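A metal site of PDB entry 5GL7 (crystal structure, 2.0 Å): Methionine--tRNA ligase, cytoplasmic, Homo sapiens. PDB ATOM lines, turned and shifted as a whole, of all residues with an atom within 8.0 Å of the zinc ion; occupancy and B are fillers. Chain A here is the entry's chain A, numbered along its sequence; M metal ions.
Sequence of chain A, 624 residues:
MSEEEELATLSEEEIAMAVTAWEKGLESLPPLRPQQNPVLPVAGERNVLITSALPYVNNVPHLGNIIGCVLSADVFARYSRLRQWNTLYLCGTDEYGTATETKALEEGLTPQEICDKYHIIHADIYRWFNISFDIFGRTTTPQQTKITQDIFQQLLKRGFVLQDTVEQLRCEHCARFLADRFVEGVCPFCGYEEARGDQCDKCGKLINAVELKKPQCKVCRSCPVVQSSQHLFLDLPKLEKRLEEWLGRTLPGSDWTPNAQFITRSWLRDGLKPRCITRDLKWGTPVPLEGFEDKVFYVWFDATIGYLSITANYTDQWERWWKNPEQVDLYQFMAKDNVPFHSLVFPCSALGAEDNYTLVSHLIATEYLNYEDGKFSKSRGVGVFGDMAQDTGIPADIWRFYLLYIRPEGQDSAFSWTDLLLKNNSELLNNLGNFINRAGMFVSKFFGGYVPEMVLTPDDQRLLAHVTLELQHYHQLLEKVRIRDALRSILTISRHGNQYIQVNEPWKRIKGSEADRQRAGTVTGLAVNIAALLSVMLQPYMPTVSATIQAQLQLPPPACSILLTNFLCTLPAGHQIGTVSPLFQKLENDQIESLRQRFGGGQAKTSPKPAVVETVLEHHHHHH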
ATOM      1  N   ARG A 170       0.554  21.411  30.908  1.00  0.00           N
ATOM      2  CA  ARG A 170      -0.553  21.237  31.833  1.00  0.00           C
ATOM      3  C   ARG A 170      -1.900  21.231  31.127  1.00  0.00           C
ATOM      4  O   ARG A 170      -2.310  22.252  30.557  1.00  0.00           O
ATOM      5  CB  ARG A 170      -0.546  22.333  32.904  1.00  0.00           C
ATOM      6  CG  ARG A 170      -1.813  22.358  33.742  1.00  0.00           C
ATOM      7  CD  ARG A 170      -1.507  22.140  35.215  1.00  0.00           C
ATOM      8  NE  ARG A 170      -2.705  22.268  36.041  1.00  0.00           N
ATOM      9  CZ  ARG A 170      -2.837  21.752  37.254  1.00  0.00           C
ATOM     10  NH1 ARG A 170      -1.840  21.059  37.799  1.00  0.00           N
ATOM     11  NH2 ARG A 170      -3.971  21.923  37.936  1.00  0.00           N
ATOM     12  N   CYS A 171      -2.571  20.083  31.149  1.00  0.00           N
ATOM     13  CA  CYS A 171      -3.953  20.023  30.696  1.00  0.00           C
ATOM     14  C   CYS A 171      -4.860  20.690  31.720  1.00  0.00           C
ATOM     15  O   CYS A 171      -5.094  20.146  32.796  1.00  0.00           O
ATOM     16  CB  CYS A 171      -4.390  18.575  30.466  1.00  0.00           C
ATOM     17  SG  CYS A 171      -6.045  18.490  29.776  1.00  0.00           S
ATOM     18  N   GLU A 172      -5.370  21.853  31.364  1.00  0.00           N
ATOM     19  CA  GLU A 172      -6.210  22.629  32.275  1.00  0.00           C
ATOM     20  C   GLU A 172      -7.593  22.002  32.402  1.00  0.00           C
ATOM     21  O   GLU A 172      -8.270  22.191  33.402  1.00  0.00           O
ATOM     22  CB  GLU A 172      -6.301  24.072  31.803  1.00  0.00           C
ATOM     23  CG  GLU A 172      -5.684  25.072  32.771  1.00  0.00           C
ATOM     24  CD  GLU A 172      -6.165  26.482  32.532  1.00  0.00           C
ATOM     25  OE1 GLU A 172      -5.482  27.234  31.811  1.00  0.00           O
ATOM     26  OE2 GLU A 172      -7.236  26.847  33.071  1.00  0.00           O
ATOM     27  N   HIS A 173      -7.993  21.247  31.379  1.00  0.00           N
ATOM     28  CA  HIS A 173      -9.263  20.524  31.434  1.00  0.00           C
ATOM     29  C   HIS A 173      -9.167  19.365  32.426  1.00  0.00           C
ATOM     30  O   HIS A 173     -10.038  19.183  33.277  1.00  0.00           O
ATOM     31  CB  HIS A 173      -9.647  20.008  30.050  1.00  0.00           C
ATOM     32  CG  HIS A 173     -11.015  19.401  29.988  1.00  0.00           C
ATOM     33  ND1 HIS A 173     -11.225  18.034  29.938  1.00  0.00           N
ATOM     34  CD2 HIS A 173     -12.239  19.966  29.974  1.00  0.00           C
ATOM     35  CE1 HIS A 173     -12.522  17.791  29.894  1.00  0.00           C
ATOM     36  NE2 HIS A 173     -13.160  18.947  29.908  1.00  0.00           N
ATOM     37  N   CYS A 174      -8.084  18.594  32.320  1.00  0.00           N
ATOM     38  CA  CYS A 174      -7.843  17.467  33.217  1.00  0.00           C
ATOM     39  C   CYS A 174      -7.325  17.960  34.573  1.00  0.00           C
ATOM     40  O   CYS A 174      -7.336  17.213  35.549  1.00  0.00           O
ATOM     41  CB  CYS A 174      -6.841  16.490  32.610  1.00  0.00           C
ATOM     42  SG  CYS A 174      -7.501  15.476  31.271  1.00  0.00           S
ATOM     43  N   ALA A 175      -6.902  19.221  34.605  1.00  0.00           N
ATOM     44  CA  ALA A 175      -6.365  19.864  35.812  1.00  0.00           C
ATOM     45  C   ALA A 175      -5.170  19.126  36.394  1.00  0.00           C
ATOM     46  O   ALA A 175      -5.163  18.747  37.565  1.00  0.00           O
ATOM     47  CB  ALA A 175      -7.459  19.991  36.865  1.00  0.00           C
ATOM     48  N   ARG A 176      -4.137  18.922  35.566  1.00  0.00           N
ATOM     49  CA  ARG A 176      -2.906  18.283  36.012  1.00  0.00           C
ATOM     50  C   ARG A 176      -1.777  18.485  35.014  1.00  0.00           C
ATOM     51  O   ARG A 176      -2.004  18.853  33.860  1.00  0.00           O
ATOM     52  CB  ARG A 176      -3.130  16.785  36.243  1.00  0.00           C
ATOM     53  CG  ARG A 176      -3.159  15.964  34.961  1.00  0.00           C
ATOM     54  CD  ARG A 176      -3.400  14.490  35.258  1.00  0.00           C
ATOM     55  NE  ARG A 176      -2.950  13.641  34.160  1.00  0.00           N
ATOM     56  CZ  ARG A 176      -3.365  12.396  33.977  1.00  0.00           C
ATOM     57  NH1 ARG A 176      -4.251  11.854  34.809  1.00  0.00           N
ATOM     58  NH2 ARG A 176      -2.900  11.683  32.954  1.00  0.00           N
ATOM     59  N   LEU A 178       1.028  17.024  32.548  1.00  0.00           N
ATOM     60  CA  LEU A 178       1.069  15.841  31.710  1.00  0.00           C
ATOM     61  C   LEU A 178       2.451  15.198  31.641  1.00  0.00           C
ATOM     62  O   LEU A 178       3.456  15.885  31.476  1.00  0.00           O
ATOM     63  CB  LEU A 178       0.609  16.187  30.290  1.00  0.00           C
ATOM     64  CG  LEU A 178      -0.868  16.551  30.104  1.00  0.00           C
ATOM     65  CD1 LEU A 178      -1.149  16.851  28.645  1.00  0.00           C
ATOM     66  CD2 LEU A 178      -1.756  15.432  30.599  1.00  0.00           C
ATOM     67  N   PHE A 182       1.372  10.948  27.901  1.00  0.00           N
ATOM     68  CA  PHE A 182       0.019  11.423  27.614  1.00  0.00           C
ATOM     69  C   PHE A 182      -0.002  12.648  26.705  1.00  0.00           C
ATOM     70  O   PHE A 182      -1.033  13.324  26.606  1.00  0.00           O
ATOM     71  CB  PHE A 182      -0.703  11.735  28.923  1.00  0.00           C
ATOM     72  CG  PHE A 182      -0.840  10.550  29.830  1.00  0.00           C
ATOM     73  CD1 PHE A 182      -1.306   9.342  29.349  1.00  0.00           C
ATOM     74  CD2 PHE A 182      -0.491  10.630  31.165  1.00  0.00           C
ATOM     75  CE1 PHE A 182      -1.440   8.242  30.181  1.00  0.00           C
ATOM     76  CE2 PHE A 182      -0.609   9.545  32.003  1.00  0.00           C
ATOM     77  CZ  PHE A 182      -1.092   8.346  31.512  1.00  0.00           C
ATOM     78  N   GLN A 216      -1.218  18.246  22.230  1.00  0.00           N
ATOM     79  CA  GLN A 216      -2.555  17.766  22.551  1.00  0.00           C
ATOM     80  C   GLN A 216      -2.506  16.719  23.655  1.00  0.00           C
ATOM     81  O   GLN A 216      -1.632  15.849  23.660  1.00  0.00           O
ATOM     82  CB  GLN A 216      -3.229  17.202  21.301  1.00  0.00           C
ATOM     83  CG  GLN A 216      -4.729  17.028  21.419  1.00  0.00           C
ATOM     84  CD  GLN A 216      -5.377  16.619  20.114  1.00  0.00           C
ATOM     85  OE1 GLN A 216      -4.695  16.278  19.148  1.00  0.00           O
ATOM     86  NE2 GLN A 216      -6.703  16.662  20.065  1.00  0.00           N
ATOM     87  N   CYS A 217      -3.448  16.791  24.585  1.00  0.00           N
ATOM     88  CA  CYS A 217      -3.560  15.803  25.639  1.00  0.00           C
ATOM     89  C   CYS A 217      -4.218  14.540  25.113  1.00  0.00           C
ATOM     90  O   CYS A 217      -5.284  14.601  24.489  1.00  0.00           O
ATOM     91  CB  CYS A 217      -4.347  16.362  26.829  1.00  0.00           C
ATOM     92  SG  CYS A 217      -4.902  15.119  28.014  1.00  0.00           S
ATOM     93  N   LYS A 218      -3.592  13.388  25.333  1.00  0.00           N
ATOM     94  CA  LYS A 218      -4.103  12.127  24.802  1.00  0.00           C
ATOM     95  C   LYS A 218      -5.460  11.759  25.396  1.00  0.00           C
ATOM     96  O   LYS A 218      -6.238  11.024  24.779  1.00  0.00           O
ATOM     97  CB  LYS A 218      -3.108  10.997  25.067  1.00  0.00           C
ATOM     98  CG  LYS A 218      -1.871  11.041  24.180  1.00  0.00           C
ATOM     99  CD  LYS A 218      -1.110   9.730  24.229  1.00  0.00           C
ATOM    100  CE  LYS A 218      -1.186   8.990  22.910  1.00  0.00           C
ATOM    101  NZ  LYS A 218      -2.553   9.045  22.318  1.00  0.00           N
ATOM    102  N   VAL A 219      -5.754  12.269  26.584  1.00  0.00           N
ATOM    103  CA  VAL A 219      -6.963  11.887  27.316  1.00  0.00           C
ATOM    104  C   VAL A 219      -8.205  12.653  26.862  1.00  0.00           C
ATOM    105  O   VAL A 219      -9.162  12.046  26.376  1.00  0.00           O
ATOM    106  CB  VAL A 219      -6.782  12.082  28.828  1.00  0.00           C
ATOM    107  CG1 VAL A 219      -8.071  11.765  29.563  1.00  0.00           C
ATOM    108  CG2 VAL A 219      -5.632  11.223  29.344  1.00  0.00           C
ATOM    109  N   CYS A 220      -8.194  13.966  27.020  1.00  0.00           N
ATOM    110  CA  CYS A 220      -9.373  14.778  26.743  1.00  0.00           C
ATOM    111  C   CYS A 220      -9.272  15.519  25.408  1.00  0.00           C
ATOM    112  O   CYS A 220     -10.228  16.185  24.996  1.00  0.00           O
ATOM    113  CB  CYS A 220      -9.588  15.790  27.864  1.00  0.00           C
ATOM    114  SG  CYS A 220      -8.407  17.153  27.823  1.00  0.00           S
ATOM    115  N   ARG A 221      -8.117  15.400  24.758  1.00  0.00           N
ATOM    116  CA  ARG A 221      -7.874  15.961  23.423  1.00  0.00           C
ATOM    117  C   ARG A 221      -7.828  17.491  23.395  1.00  0.00           C
ATOM    118  O   ARG A 221      -7.840  18.089  22.315  1.00  0.00           O
ATOM    119  CB  ARG A 221      -8.918  15.457  22.423  1.00  0.00           C
ATOM    120  CG  ARG A 221      -9.071  13.944  22.393  1.00  0.00           C
ATOM    121  CD  ARG A 221      -7.769  13.265  22.028  1.00  0.00           C
ATOM    122  NE  ARG A 221      -7.604  13.139  20.586  1.00  0.00           N
ATOM    123  CZ  ARG A 221      -6.457  12.852  19.979  1.00  0.00           C
ATOM    124  NH1 ARG A 221      -5.349  12.668  20.701  1.00  0.00           N
ATOM    125  NH2 ARG A 221      -6.407  12.752  18.663  1.00  0.00           N
ATOM    126  N   SER A 222      -7.757  18.125  24.563  1.00  0.00           N
ATOM    127  CA  SER A 222      -7.638  19.577  24.612  1.00  0.00           C
ATOM    128  C   SER A 222      -6.191  20.019  24.375  1.00  0.00           C
ATOM    129  O   SER A 222      -5.329  19.196  24.084  1.00  0.00           O
ATOM    130  CB  SER A 222      -8.137  20.117  25.950  1.00  0.00           C
ATOM    131  OG  SER A 222      -7.272  19.752  27.017  1.00  0.00           O
ATOM    132  N   CYS A 223      -5.943  21.311  24.516  1.00  0.00           N
ATOM    133  CA  CYS A 223      -4.617  21.871  24.274  1.00  0.00           C
ATOM    134  C   CYS A 223      -3.917  22.268  25.575  1.00  0.00           C
ATOM    135  O   CYS A 223      -4.296  23.235  26.220  1.00  0.00           O
ATOM    136  CB  CYS A 223      -4.698  23.078  23.352  1.00  0.00           C
ATOM    137  SG  CYS A 223      -5.387  22.724  21.728  1.00  0.00           S
ATOM    138  N   PRO A 224      -2.878  21.505  25.958  1.00  0.00           N
ATOM    139  CA  PRO A 224      -2.079  21.782  27.152  1.00  0.00           C
ATOM    140  C   PRO A 224      -1.316  23.100  27.020  1.00  0.00           C
ATOM    141  O   PRO A 224      -1.014  23.527  25.901  1.00  0.00           O
ATOM    142  CB  PRO A 224      -1.113  20.602  27.226  1.00  0.00           C
ATOM    143  CG  PRO A 224      -1.676  19.557  26.322  1.00  0.00           C
ATOM    144  CD  PRO A 224      -2.410  20.296  25.256  1.00  0.00           C
HETATM  145 ZN    ZN M   1      -6.474  16.412  29.243  1.00  0.00          ZN
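SG of Cys 220 lies close to OG of Ser 222 (2.9 Å).
The side-chain sulfur (SG) of Cys 171 sits close to the side-chain hydroxyl (OG) of Ser 222 (3.3 Å).
The side-chain sulfur (SG) of Cys 217 sits close to the backbone NH (N) of Val 219, at 3.3 Å.
N of Cys 217 sits at hydrogen-bond distance from O of Ser 222, 3.1 Å away.
The backbone NH (N) of Cys 171 sits at hydrogen-bond distance from the backbone carbonyl oxygen (O) of Arg 176 (3.0 Å).
The side-chain sulfur (SG) of Cys 171 lies close to the backbone NH (N) of His 173, 3.7 Å away.
The side-chain sulfur (SG) of Cys 220 lies close to a ring nitrogen (ND1) of His 173, 3.6 Å away.
Within 4 Å of the zinc ion: Cys 171, Cys 174, Cys 217 and Cys 220.
The zinc ion is bound by SG of Cys 171, 2.2 Å away.
The zinc ion is bound by SG of Cys 217.
SG of Cys 174 is bound to the zinc ion (2.5 Å).
The zinc ion is bound by SG of Cys 220.
The zinc ion has four donor atoms within binding distance.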
